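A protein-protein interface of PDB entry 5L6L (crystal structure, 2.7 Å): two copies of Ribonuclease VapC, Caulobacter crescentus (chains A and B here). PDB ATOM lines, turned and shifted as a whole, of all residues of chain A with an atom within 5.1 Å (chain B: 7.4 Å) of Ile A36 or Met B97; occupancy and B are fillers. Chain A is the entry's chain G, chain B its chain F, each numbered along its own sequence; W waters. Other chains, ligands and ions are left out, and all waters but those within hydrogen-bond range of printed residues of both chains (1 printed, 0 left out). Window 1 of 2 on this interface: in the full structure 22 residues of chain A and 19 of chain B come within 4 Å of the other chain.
The backbone NH (N) of Ala B75 is in hydrogen-bond range of the side-chain carboxylate (OD1) of Asp B72, 3.3 Å away. The side-chain hydroxyl (OG) of Ser A34 sits at hydrogen-bond distance from the backbone NH (N) of Ile A36, at 2.9 Å. The backbone NH of Ile A35 is in hydrogen-bond range of the side-chain amide oxygen of Gln A101 (3.3 Å).
Ile A35 touches Phe B71, and with the chains exchanged Phe A71 touches Ile B35. Ile A36 touches Met B97, but with the chains exchanged Met A97 does not touch Ile B36 (4.3 Å). Phe A71 touches its own counterpart, Phe B71. Positions printed for both chains: 34, 35, 36, 71, 94, 97, 98 and 101.
Of the 24 printed residues of chain B, 6 touch a printed residue of chain A. Of the 13 printed residues of chain A, 5 touch a printed residue of chain B. Hydrophobic or aromatic side chains of chain A that line the printed part of chain B: Ile A35, Ile A36, Val A39 and Phe A71. Along chain A the printed residues that touch a printed residue of chain B span positions 35 to 71. Among the printed residues, 10 pairs touch across the chains. Among the printed residues, no Asp or Glu carboxylate lies within 4 Å of a Lys or Arg side-chain nitrogen of the other chain.
Among the printed residues, merely in contact across the chains: Ile A35 with Asp B72, Val A39 with Tyr B79, Arg A38 with Ala B76, Ile A36 with Met B97, Val A39 with Phe B71, Ile A35 with Phe B71, Phe A71 with Ile B35, Ile A35 with Ala B76 and Val A39 with Met B97.
Water W1 lies within hydrogen-bond range of the side-chain hydroxyl of Tyr B79 (2.6 Å) and the backbone carbonyl oxygen of Val A39 (3.2 Å).
Ile A36 touches one residue of chain B. Printed residues of chain B within 4 Å of Arg A38: Ala B76. Of the printed residues of chain B, Val A39 touches Phe B71 (3.5 Å), Tyr B79 (3.3 Å) and Met B97 (3.8 Å). Of the printed residues of chain A, Ile B35 touches Phe A71 (3.7 Å). Of the printed residues of chain A, Ala B76 touches Ile A35 (3.8 Å) and Arg A38 (3.4 Å). Of the printed residues of chain A, Met B97 touches Ile A36 and Val A39.
O of Phe B71 sits at hydrogen-bond distance from N of Phe A71 (2.8 Å).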
ATOM      1  N   THR A   7      31.951  32.112  13.636  1.00  0.00           N
ATOM      2  CA  THR A   7      31.510  33.161  14.543  1.00  0.00           C
ATOM      3  C   THR A   7      32.068  34.524  14.148  1.00  0.00           C
ATOM      4  O   THR A   7      31.366  35.532  14.260  1.00  0.00           O
ATOM      5  CB  THR A   7      31.897  32.803  15.974  1.00  0.00           C
ATOM      6  OG1 THR A   7      31.077  31.714  16.388  1.00  0.00           O
ATOM      7  CG2 THR A   7      31.703  33.991  16.946  1.00  0.00           C
ATOM      8  N   SER A  34      25.874  28.021  13.886  1.00  0.00           N
ATOM      9  CA  SER A  34      26.008  27.152  15.047  1.00  0.00           C
ATOM     10  C   SER A  34      25.414  27.827  16.272  1.00  0.00           C
ATOM     11  O   SER A  34      25.565  29.036  16.450  1.00  0.00           O
ATOM     12  CB  SER A  34      27.474  26.852  15.310  1.00  0.00           C
ATOM     13  OG  SER A  34      27.655  26.549  16.670  1.00  0.00           O
ATOM     14  N   ILE A  35      24.733  27.051  17.125  1.00  0.00           N
ATOM     15  CA  ILE A  35      24.212  27.641  18.361  1.00  0.00           C
ATOM     16  C   ILE A  35      25.337  28.067  19.283  1.00  0.00           C
ATOM     17  O   ILE A  35      25.152  28.983  20.090  1.00  0.00           O
ATOM     18  CB  ILE A  35      23.252  26.723  19.140  1.00  0.00           C
ATOM     19  CG1 ILE A  35      22.547  27.544  20.226  1.00  0.00           C
ATOM     20  CG2 ILE A  35      23.989  25.521  19.752  1.00  0.00           C
ATOM     21  CD1 ILE A  35      21.056  27.318  20.292  1.00  0.00           C
ATOM     22  N   ILE A  36      26.511  27.446  19.179  1.00  0.00           N
ATOM     23  CA  ILE A  36      27.646  27.978  19.916  1.00  0.00           C
ATOM     24  C   ILE A  36      27.944  29.395  19.457  1.00  0.00           C
ATOM     25  O   ILE A  36      28.350  30.245  20.256  1.00  0.00           O
ATOM     26  CB  ILE A  36      28.867  27.051  19.759  1.00  0.00           C
ATOM     27  CG1 ILE A  36      28.493  25.656  20.240  1.00  0.00           C
ATOM     28  CG2 ILE A  36      30.042  27.554  20.573  1.00  0.00           C
ATOM     29  CD1 ILE A  36      27.869  25.675  21.603  1.00  0.00           C
ATOM     30  N   SER A  37      27.721  29.681  18.172  1.00  0.00           N
ATOM     31  CA  SER A  37      27.963  31.026  17.676  1.00  0.00           C
ATOM     32  C   SER A  37      26.917  31.986  18.205  1.00  0.00           C
ATOM     33  O   SER A  37      27.242  33.130  18.556  1.00  0.00           O
ATOM     34  CB  SER A  37      28.008  31.038  16.148  1.00  0.00           C
ATOM     35  OG  SER A  37      29.164  30.345  15.693  1.00  0.00           O
ATOM     36  N   ARG A  38      25.667  31.525  18.312  1.00  0.00           N
ATOM     37  CA  ARG A  38      24.626  32.370  18.880  1.00  0.00           C
ATOM     38  C   ARG A  38      25.018  32.820  20.279  1.00  0.00           C
ATOM     39  O   ARG A  38      24.954  34.012  20.599  1.00  0.00           O
ATOM     40  CB  ARG A  38      23.288  31.635  18.903  1.00  0.00           C
ATOM     41  CG  ARG A  38      22.107  32.578  19.122  1.00  0.00           C
ATOM     42  CD  ARG A  38      20.787  31.906  19.580  1.00  0.00           C
ATOM     43  NE  ARG A  38      20.061  32.775  20.499  1.00  0.00           N
ATOM     44  CZ  ARG A  38      18.948  32.437  21.139  1.00  0.00           C
ATOM     45  NH1 ARG A  38      18.427  31.226  20.958  1.00  0.00           N
ATOM     46  NH2 ARG A  38      18.356  33.304  21.977  1.00  0.00           N
ATOM     47  N   VAL A  39      25.493  31.881  21.109  1.00  0.00           N
ATOM     48  CA  VAL A  39      25.859  32.224  22.473  1.00  0.00           C
ATOM     49  C   VAL A  39      26.941  33.295  22.478  1.00  0.00           C
ATOM     50  O   VAL A  39      26.825  34.296  23.193  1.00  0.00           O
ATOM     51  CB  VAL A  39      26.288  30.972  23.259  1.00  0.00           C
ATOM     52  CG1 VAL A  39      26.900  31.365  24.608  1.00  0.00           C
ATOM     53  CG2 VAL A  39      25.103  30.082  23.493  1.00  0.00           C
ATOM     54  N   GLU A  40      28.003  33.104  21.683  1.00  0.00           N
ATOM     55  CA  GLU A  40      29.043  34.129  21.557  1.00  0.00           C
ATOM     56  C   GLU A  40      28.463  35.453  21.069  1.00  0.00           C
ATOM     57  O   GLU A  40      28.865  36.530  21.530  1.00  0.00           O
ATOM     58  CB  GLU A  40      30.144  33.681  20.588  1.00  0.00           C
ATOM     59  CG  GLU A  40      30.924  32.430  20.958  1.00  0.00           C
ATOM     60  CD  GLU A  40      32.172  32.236  20.072  1.00  0.00           C
ATOM     61  OE1 GLU A  40      32.016  31.631  18.984  1.00  0.00           O
ATOM     62  OE2 GLU A  40      33.301  32.675  20.458  1.00  0.00           O
ATOM     63  N   PHE A  71      22.776  22.011  19.379  1.00  0.00           N
ATOM     64  CA  PHE A  71      23.963  21.182  19.561  1.00  0.00           C
ATOM     65  C   PHE A  71      23.530  19.826  20.109  1.00  0.00           C
ATOM     66  O   PHE A  71      23.097  19.708  21.261  1.00  0.00           O
ATOM     67  CB  PHE A  71      24.997  21.850  20.465  1.00  0.00           C
ATOM     68  CG  PHE A  71      26.347  21.215  20.358  1.00  0.00           C
ATOM     69  CD1 PHE A  71      27.282  21.693  19.446  1.00  0.00           C
ATOM     70  CD2 PHE A  71      26.662  20.075  21.123  1.00  0.00           C
ATOM     71  CE1 PHE A  71      28.530  21.077  19.338  1.00  0.00           C
ATOM     72  CE2 PHE A  71      27.898  19.462  21.015  1.00  0.00           C
ATOM     73  CZ  PHE A  71      28.835  19.963  20.128  1.00  0.00           C
ATOM     74  N   VAL A  94      35.862  25.639  21.441  1.00  0.00           N
ATOM     75  CA  VAL A  94      34.716  26.393  20.905  1.00  0.00           C
ATOM     76  C   VAL A  94      34.658  26.299  19.386  1.00  0.00           C
ATOM     77  O   VAL A  94      33.602  26.009  18.809  1.00  0.00           O
ATOM     78  CB  VAL A  94      34.742  27.867  21.348  1.00  0.00           C
ATOM     79  CG1 VAL A  94      33.701  28.638  20.583  1.00  0.00           C
ATOM     80  CG2 VAL A  94      34.462  28.014  22.819  1.00  0.00           C
ATOM     81  N   MET A  97      33.721  22.755  18.374  1.00  0.00           N
ATOM     82  CA  MET A  97      32.301  22.528  18.554  1.00  0.00           C
ATOM     83  C   MET A  97      31.529  23.074  17.363  1.00  0.00           C
ATOM     84  O   MET A  97      30.703  22.369  16.786  1.00  0.00           O
ATOM     85  CB  MET A  97      31.803  23.170  19.833  1.00  0.00           C
ATOM     86  CG  MET A  97      32.071  22.316  21.022  1.00  0.00           C
ATOM     87  SD  MET A  97      31.279  23.039  22.631  1.00  0.00           S
ATOM     88  CE  MET A  97      32.183  24.753  22.561  1.00  0.00           C
ATOM     89  N   ILE A  98      31.813  24.334  17.009  1.00  0.00           N
ATOM     90  CA  ILE A  98      31.178  24.956  15.845  1.00  0.00           C
ATOM     91  C   ILE A  98      31.394  24.100  14.608  1.00  0.00           C
ATOM     92  O   ILE A  98      30.435  23.649  13.968  1.00  0.00           O
ATOM     93  CB  ILE A  98      31.712  26.377  15.632  1.00  0.00           C
ATOM     94  CG1 ILE A  98      31.099  27.321  16.642  1.00  0.00           C
ATOM     95  CG2 ILE A  98      31.409  26.868  14.237  1.00  0.00           C
ATOM     96  CD1 ILE A  98      31.995  28.453  16.928  1.00  0.00           C
ATOM     97  N   GLN A 101      29.393  21.041  14.175  1.00  0.00           N
ATOM     98  CA  GLN A 101      28.015  21.143  13.700  1.00  0.00           C
ATOM     99  C   GLN A 101      27.966  21.239  12.184  1.00  0.00           C
ATOM    100  O   GLN A 101      27.148  20.568  11.557  1.00  0.00           O
ATOM    101  CB  GLN A 101      27.300  22.340  14.336  1.00  0.00           C
ATOM    102  CG  GLN A 101      27.337  22.291  15.832  1.00  0.00           C
ATOM    103  CD  GLN A 101      26.324  23.198  16.480  1.00  0.00           C
ATOM    104  OE1 GLN A 101      26.618  24.351  16.773  1.00  0.00           O
ATOM    105  NE2 GLN A 101      25.116  22.673  16.732  1.00  0.00           N
ATOM    106  N   SER B  34      24.591  18.023  31.076  1.00  0.00           N
ATOM    107  CA  SER B  34      24.631  18.921  29.934  1.00  0.00           C
ATOM    108  C   SER B  34      25.546  18.382  28.840  1.00  0.00           C
ATOM    109  O   SER B  34      26.624  17.843  29.112  1.00  0.00           O
ATOM    110  CB  SER B  34      25.115  20.301  30.350  1.00  0.00           C
ATOM    111  OG  SER B  34      25.443  21.071  29.193  1.00  0.00           O
ATOM    112  N   ILE B  35      25.134  18.572  27.586  1.00  0.00           N
ATOM    113  CA  ILE B  35      25.976  18.132  26.482  1.00  0.00           C
ATOM    114  C   ILE B  35      27.234  18.976  26.387  1.00  0.00           C
ATOM    115  O   ILE B  35      28.250  18.508  25.882  1.00  0.00           O
ATOM    116  CB  ILE B  35      25.198  18.131  25.151  1.00  0.00           C
ATOM    117  CG1 ILE B  35      25.879  17.183  24.146  1.00  0.00           C
ATOM    118  CG2 ILE B  35      25.007  19.565  24.637  1.00  0.00           C
ATOM    119  CD1 ILE B  35      25.157  17.019  22.863  1.00  0.00           C
ATOM    120  N   ILE B  36      27.228  20.192  26.917  1.00  0.00           N
ATOM    121  CA  ILE B  36      28.489  20.913  27.056  1.00  0.00           C
ATOM    122  C   ILE B  36      29.444  20.126  27.946  1.00  0.00           C
ATOM    123  O   ILE B  36      30.626  19.957  27.625  1.00  0.00           O
ATOM    124  CB  ILE B  36      28.244  22.333  27.587  1.00  0.00           C
ATOM    125  CG1 ILE B  36      27.306  23.074  26.627  1.00  0.00           C
ATOM    126  CG2 ILE B  36      29.556  23.058  27.755  1.00  0.00           C
ATOM    127  CD1 ILE B  36      27.736  23.071  25.098  1.00  0.00           C
ATOM    128  N   PHE B  71      22.058  21.396  23.896  1.00  0.00           N
ATOM    129  CA  PHE B  71      22.080  22.855  23.975  1.00  0.00           C
ATOM    130  C   PHE B  71      21.350  23.428  22.771  1.00  0.00           C
ATOM    131  O   PHE B  71      21.853  23.371  21.649  1.00  0.00           O
ATOM    132  CB  PHE B  71      23.490  23.431  24.037  1.00  0.00           C
ATOM    133  CG  PHE B  71      23.504  24.844  24.573  1.00  0.00           C
ATOM    134  CD1 PHE B  71      23.278  25.925  23.730  1.00  0.00           C
ATOM    135  CD2 PHE B  71      23.641  25.081  25.949  1.00  0.00           C
ATOM    136  CE1 PHE B  71      23.243  27.206  24.243  1.00  0.00           C
ATOM    137  CE2 PHE B  71      23.610  26.367  26.464  1.00  0.00           C
ATOM    138  CZ  PHE B  71      23.415  27.426  25.621  1.00  0.00           C
ATOM    139  N   ASP B  72      20.193  24.020  23.009  1.00  0.00           N
ATOM    140  CA  ASP B  72      19.284  24.433  21.957  1.00  0.00           C
ATOM    141  C   ASP B  72      18.811  25.877  22.207  1.00  0.00           C
ATOM    142  O   ASP B  72      19.218  26.539  23.171  1.00  0.00           O
ATOM    143  CB  ASP B  72      18.105  23.453  21.888  1.00  0.00           C
ATOM    144  CG  ASP B  72      17.417  23.283  23.254  1.00  0.00           C
ATOM    145  OD1 ASP B  72      17.735  24.074  24.162  1.00  0.00           O
ATOM    146  OD2 ASP B  72      16.563  22.387  23.431  1.00  0.00           O
ATOM    147  N   ALA B  75      17.878  26.960  25.800  1.00  0.00           N
ATOM    148  CA  ALA B  75      19.026  27.244  26.658  1.00  0.00           C
ATOM    149  C   ALA B  75      19.748  28.527  26.234  1.00  0.00           C
ATOM    150  O   ALA B  75      20.188  29.304  27.085  1.00  0.00           O
ATOM    151  CB  ALA B  75      19.995  26.057  26.676  1.00  0.00           C
ATOM    152  N   ALA B  76      19.884  28.775  24.930  1.00  0.00           N
ATOM    153  CA  ALA B  76      20.504  30.030  24.497  1.00  0.00           C
ATOM    154  C   ALA B  76      19.642  31.254  24.828  1.00  0.00           C
ATOM    155  O   ALA B  76      20.171  32.359  24.935  1.00  0.00           O
ATOM    156  CB  ALA B  76      20.791  29.996  23.005  1.00  0.00           C
ATOM    157  N   GLU B  78      18.071  31.328  27.737  1.00  0.00           N
ATOM    158  CA  GLU B  78      18.410  31.472  29.141  1.00  0.00           C
ATOM    159  C   GLU B  78      19.768  32.128  29.294  1.00  0.00           C
ATOM    160  O   GLU B  78      19.971  32.962  30.189  1.00  0.00           O
ATOM    161  CB  GLU B  78      18.368  30.103  29.825  1.00  0.00           C
ATOM    162  CG  GLU B  78      16.994  29.503  29.875  1.00  0.00           C
ATOM    163  CD  GLU B  78      16.058  30.287  30.785  1.00  0.00           C
ATOM    164  OE1 GLU B  78      14.874  29.886  30.924  1.00  0.00           O
ATOM    165  OE2 GLU B  78      16.516  31.306  31.364  1.00  0.00           O
ATOM    166  N   TYR B  79      20.705  31.775  28.417  1.00  0.00           N
ATOM    167  CA  TYR B  79      22.025  32.373  28.497  1.00  0.00           C
ATOM    168  C   TYR B  79      21.934  33.870  28.277  1.00  0.00           C
ATOM    169  O   TYR B  79      22.548  34.654  29.020  1.00  0.00           O
ATOM    170  CB  TYR B  79      22.973  31.740  27.478  1.00  0.00           C
ATOM    171  CG  TYR B  79      24.299  32.456  27.397  1.00  0.00           C
ATOM    172  CD1 TYR B  79      25.291  32.232  28.341  1.00  0.00           C
ATOM    173  CD2 TYR B  79      24.556  33.372  26.394  1.00  0.00           C
ATOM    174  CE1 TYR B  79      26.508  32.898  28.281  1.00  0.00           C
ATOM    175  CE2 TYR B  79      25.751  34.040  26.327  1.00  0.00           C
ATOM    176  CZ  TYR B  79      26.728  33.800  27.267  1.00  0.00           C
ATOM    177  OH  TYR B  79      27.945  34.446  27.210  1.00  0.00           O
ATOM    178  N   ILE B  82      20.860  35.629  31.207  1.00  0.00           N
ATOM    179  CA  ILE B  82      21.872  35.720  32.259  1.00  0.00           C
ATOM    180  C   ILE B  82      22.802  36.891  31.994  1.00  0.00           C
ATOM    181  O   ILE B  82      23.135  37.663  32.903  1.00  0.00           O
ATOM    182  CB  ILE B  82      22.673  34.418  32.399  1.00  0.00           C
ATOM    183  CG1 ILE B  82      21.803  33.267  32.923  1.00  0.00           C
ATOM    184  CG2 ILE B  82      23.854  34.660  33.353  1.00  0.00           C
ATOM    185  CD1 ILE B  82      22.448  31.905  32.762  1.00  0.00           C
ATOM    186  N   LYS B  92      33.045  33.115  32.444  1.00  0.00           N
ATOM    187  CA  LYS B  92      31.907  32.311  32.877  1.00  0.00           C
ATOM    188  C   LYS B  92      30.968  31.901  31.728  1.00  0.00           C
ATOM    189  O   LYS B  92      29.874  31.396  31.994  1.00  0.00           O
ATOM    190  CB  LYS B  92      31.128  33.047  33.987  1.00  0.00           C
ATOM    191  CG  LYS B  92      32.011  33.576  35.154  1.00  0.00           C
ATOM    192  CD  LYS B  92      31.332  33.623  36.512  1.00  0.00           C
ATOM    193  CE  LYS B  92      30.490  34.869  36.676  1.00  0.00           C
ATOM    194  NZ  LYS B  92      29.883  34.960  38.041  1.00  0.00           N
ATOM    195  N   VAL B  93      31.378  32.065  30.463  1.00  0.00           N
ATOM    196  CA  VAL B  93      30.516  31.670  29.344  1.00  0.00           C
ATOM    197  C   VAL B  93      30.131  30.196  29.455  1.00  0.00           C
ATOM    198  O   VAL B  93      28.946  29.847  29.454  1.00  0.00           O
ATOM    199  CB  VAL B  93      31.191  31.959  27.988  1.00  0.00           C
ATOM    200  CG1 VAL B  93      30.343  31.415  26.834  1.00  0.00           C
ATOM    201  CG2 VAL B  93      31.446  33.438  27.810  1.00  0.00           C
ATOM    202  N   VAL B  94      31.127  29.307  29.528  1.00  0.00           N
ATOM    203  CA  VAL B  94      30.827  27.882  29.465  1.00  0.00           C
ATOM    204  C   VAL B  94      29.913  27.475  30.614  1.00  0.00           C
ATOM    205  O   VAL B  94      28.852  26.872  30.395  1.00  0.00           O
ATOM    206  CB  VAL B  94      32.114  27.050  29.457  1.00  0.00           C
ATOM    207  CG1 VAL B  94      31.775  25.596  29.818  1.00  0.00           C
ATOM    208  CG2 VAL B  94      32.804  27.146  28.100  1.00  0.00           C
ATOM    209  N   ASP B  95      30.300  27.821  31.860  1.00  0.00           N
ATOM    210  CA  ASP B  95      29.471  27.476  33.017  1.00  0.00           C
ATOM    211  C   ASP B  95      28.082  28.106  32.915  1.00  0.00           C
ATOM    212  O   ASP B  95      27.096  27.531  33.394  1.00  0.00           O
ATOM    213  CB  ASP B  95      30.145  27.899  34.321  1.00  0.00           C
ATOM    214  CG  ASP B  95      31.367  27.036  34.699  1.00  0.00           C
ATOM    215  OD1 ASP B  95      31.431  25.833  34.338  1.00  0.00           O
ATOM    216  OD2 ASP B  95      32.271  27.570  35.399  1.00  0.00           O
ATOM    217  N   ARG B  96      27.964  29.256  32.257  1.00  0.00           N
ATOM    218  CA  ARG B  96      26.636  29.841  32.105  1.00  0.00           C
ATOM    219  C   ARG B  96      25.802  29.106  31.065  1.00  0.00           C
ATOM    220  O   ARG B  96      24.571  29.084  31.167  1.00  0.00           O
ATOM    221  CB  ARG B  96      26.749  31.324  31.770  1.00  0.00           C
ATOM    222  CG  ARG B  96      27.051  32.162  32.989  1.00  0.00           C
ATOM    223  CD  ARG B  96      27.509  33.527  32.613  1.00  0.00           C
ATOM    224  NE  ARG B  96      27.468  34.415  33.766  1.00  0.00           N
ATOM    225  CZ  ARG B  96      27.644  35.726  33.687  1.00  0.00           C
ATOM    226  NH1 ARG B  96      27.869  36.282  32.501  1.00  0.00           N
ATOM    227  NH2 ARG B  96      27.604  36.472  34.785  1.00  0.00           N
ATOM    228  N   MET B  97      26.431  28.486  30.076  1.00  0.00           N
ATOM    229  CA  MET B  97      25.665  27.690  29.143  1.00  0.00           C
ATOM    230  C   MET B  97      25.037  26.500  29.862  1.00  0.00           C
ATOM    231  O   MET B  97      23.870  26.189  29.667  1.00  0.00           O
ATOM    232  CB  MET B  97      26.551  27.224  28.016  1.00  0.00           C
ATOM    233  CG  MET B  97      26.839  28.282  26.990  1.00  0.00           C
ATOM    234  SD  MET B  97      27.956  27.584  25.605  1.00  0.00           S
ATOM    235  CE  MET B  97      26.590  26.738  24.611  1.00  0.00           C
ATOM    236  N   ILE B  98      25.842  25.855  30.707  1.00  0.00           N
ATOM    237  CA  ILE B  98      25.408  24.667  31.429  1.00  0.00           C
ATOM    238  C   ILE B  98      24.269  25.019  32.366  1.00  0.00           C
ATOM    239  O   ILE B  98      23.233  24.340  32.399  1.00  0.00           O
ATOM    240  CB  ILE B  98      26.593  24.045  32.200  1.00  0.00           C
ATOM    241  CG1 ILE B  98      27.768  23.746  31.259  1.00  0.00           C
ATOM    242  CG2 ILE B  98      26.166  22.801  32.930  1.00  0.00           C
ATOM    243  CD1 ILE B  98      28.918  22.969  31.912  1.00  0.00           C
ATOM    244  N   ALA B  99      24.449  26.086  33.153  1.00  0.00           N
ATOM    245  CA  ALA B  99      23.385  26.520  34.059  1.00  0.00           C
ATOM    246  C   ALA B  99      22.130  26.914  33.289  1.00  0.00           C
ATOM    247  O   ALA B  99      21.011  26.651  33.743  1.00  0.00           O
ATOM    248  CB  ALA B  99      23.861  27.676  34.938  1.00  0.00           C
ATOM    249  N   ALA B 100      22.298  27.517  32.104  1.00  0.00           N
ATOM    250  CA  ALA B 100      21.139  27.901  31.296  1.00  0.00           C
ATOM    251  C   ALA B 100      20.246  26.703  31.025  1.00  0.00           C
ATOM    252  O   ALA B 100      19.015  26.823  31.045  1.00  0.00           O
ATOM    253  CB  ALA B 100      21.581  28.542  29.981  1.00  0.00           C
ATOM    254  N   GLN B 101      20.847  25.531  30.790  1.00  0.00           N
ATOM    255  CA  GLN B 101      20.042  24.348  30.534  1.00  0.00           C
ATOM    256  C   GLN B 101      19.291  23.933  31.791  1.00  0.00           C
ATOM    257  O   GLN B 101      18.083  23.660  31.744  1.00  0.00           O
ATOM    258  CB  GLN B 101      20.927  23.231  30.019  1.00  0.00           C
ATOM    259  CG  GLN B 101      21.925  23.722  29.021  1.00  0.00           C
ATOM    260  CD  GLN B 101      22.586  22.581  28.282  1.00  0.00           C
ATOM    261  OE1 GLN B 101      23.804  22.399  28.367  1.00  0.00           O
ATOM    262  NE2 GLN B 101      21.783  21.804  27.539  1.00  0.00           N
ATOM    263  N   ALA B 102      19.986  23.914  32.933  1.00  0.00           N
ATOM    264  CA  ALA B 102      19.310  23.674  34.200  1.00  0.00           C
ATOM    265  C   ALA B 102      18.141  24.637  34.398  1.00  0.00           C
ATOM    266  O   ALA B 102      17.048  24.223  34.803  1.00  0.00           O
ATOM    267  CB  ALA B 102      20.311  23.781  35.344  1.00  0.00           C
ATOM    268  N   LEU B 103      18.332  25.916  34.085  1.00  0.00           N
ATOM    269  CA  LEU B 103      17.201  26.830  34.130  1.00  0.00           C
ATOM    270  C   LEU B 103      16.091  26.376  33.185  1.00  0.00           C
ATOM    271  O   LEU B 103      14.911  26.361  33.562  1.00  0.00           O
ATOM    272  CB  LEU B 103      17.645  28.244  33.773  1.00  0.00           C
ATOM    273  CG  LEU B 103      18.398  29.105  34.780  1.00  0.00           C
ATOM    274  CD1 LEU B 103      18.882  30.352  34.094  1.00  0.00           C
ATOM    275  CD2 LEU B 103      17.490  29.436  35.915  1.00  0.00           C
ATOM    276  N   PHE B 117      27.820  30.961  40.457  1.00  0.00           N
ATOM    277  CA  PHE B 117      26.498  30.897  39.867  1.00  0.00           C
ATOM    278  C   PHE B 117      25.466  31.691  40.656  1.00  0.00           C
ATOM    279  O   PHE B 117      24.282  31.688  40.296  1.00  0.00           O
ATOM    280  CB  PHE B 117      26.057  29.430  39.740  1.00  0.00           C
ATOM    281  CG  PHE B 117      27.038  28.566  38.978  1.00  0.00           C
ATOM    282  CD1 PHE B 117      28.128  27.985  39.628  1.00  0.00           C
ATOM    283  CD2 PHE B 117      26.879  28.341  37.610  1.00  0.00           C
ATOM    284  CE1 PHE B 117      29.029  27.214  38.934  1.00  0.00           C
ATOM    285  CE2 PHE B 117      27.781  27.569  36.915  1.00  0.00           C
ATOM    286  CZ  PHE B 117      28.851  27.006  37.573  1.00  0.00           C
ATOM    287  N   ILE B 120      23.164  34.129  38.637  1.00  0.00           N
ATOM    288  CA  ILE B 120      22.172  33.637  37.686  1.00  0.00           C
ATOM    289  C   ILE B 120      20.809  33.631  38.370  1.00  0.00           C
ATOM    290  O   ILE B 120      20.537  32.723  39.165  1.00  0.00           O
ATOM    291  CB  ILE B 120      22.536  32.221  37.206  1.00  0.00           C
ATOM    292  CG1 ILE B 120      23.836  32.209  36.405  1.00  0.00           C
ATOM    293  CG2 ILE B 120      21.434  31.652  36.375  1.00  0.00           C
ATOM    294  CD1 ILE B 120      24.684  31.017  36.652  1.00  0.00           C
HETATM  295  O   HOH W   1      29.316  34.989  25.122  1.00  0.00           O
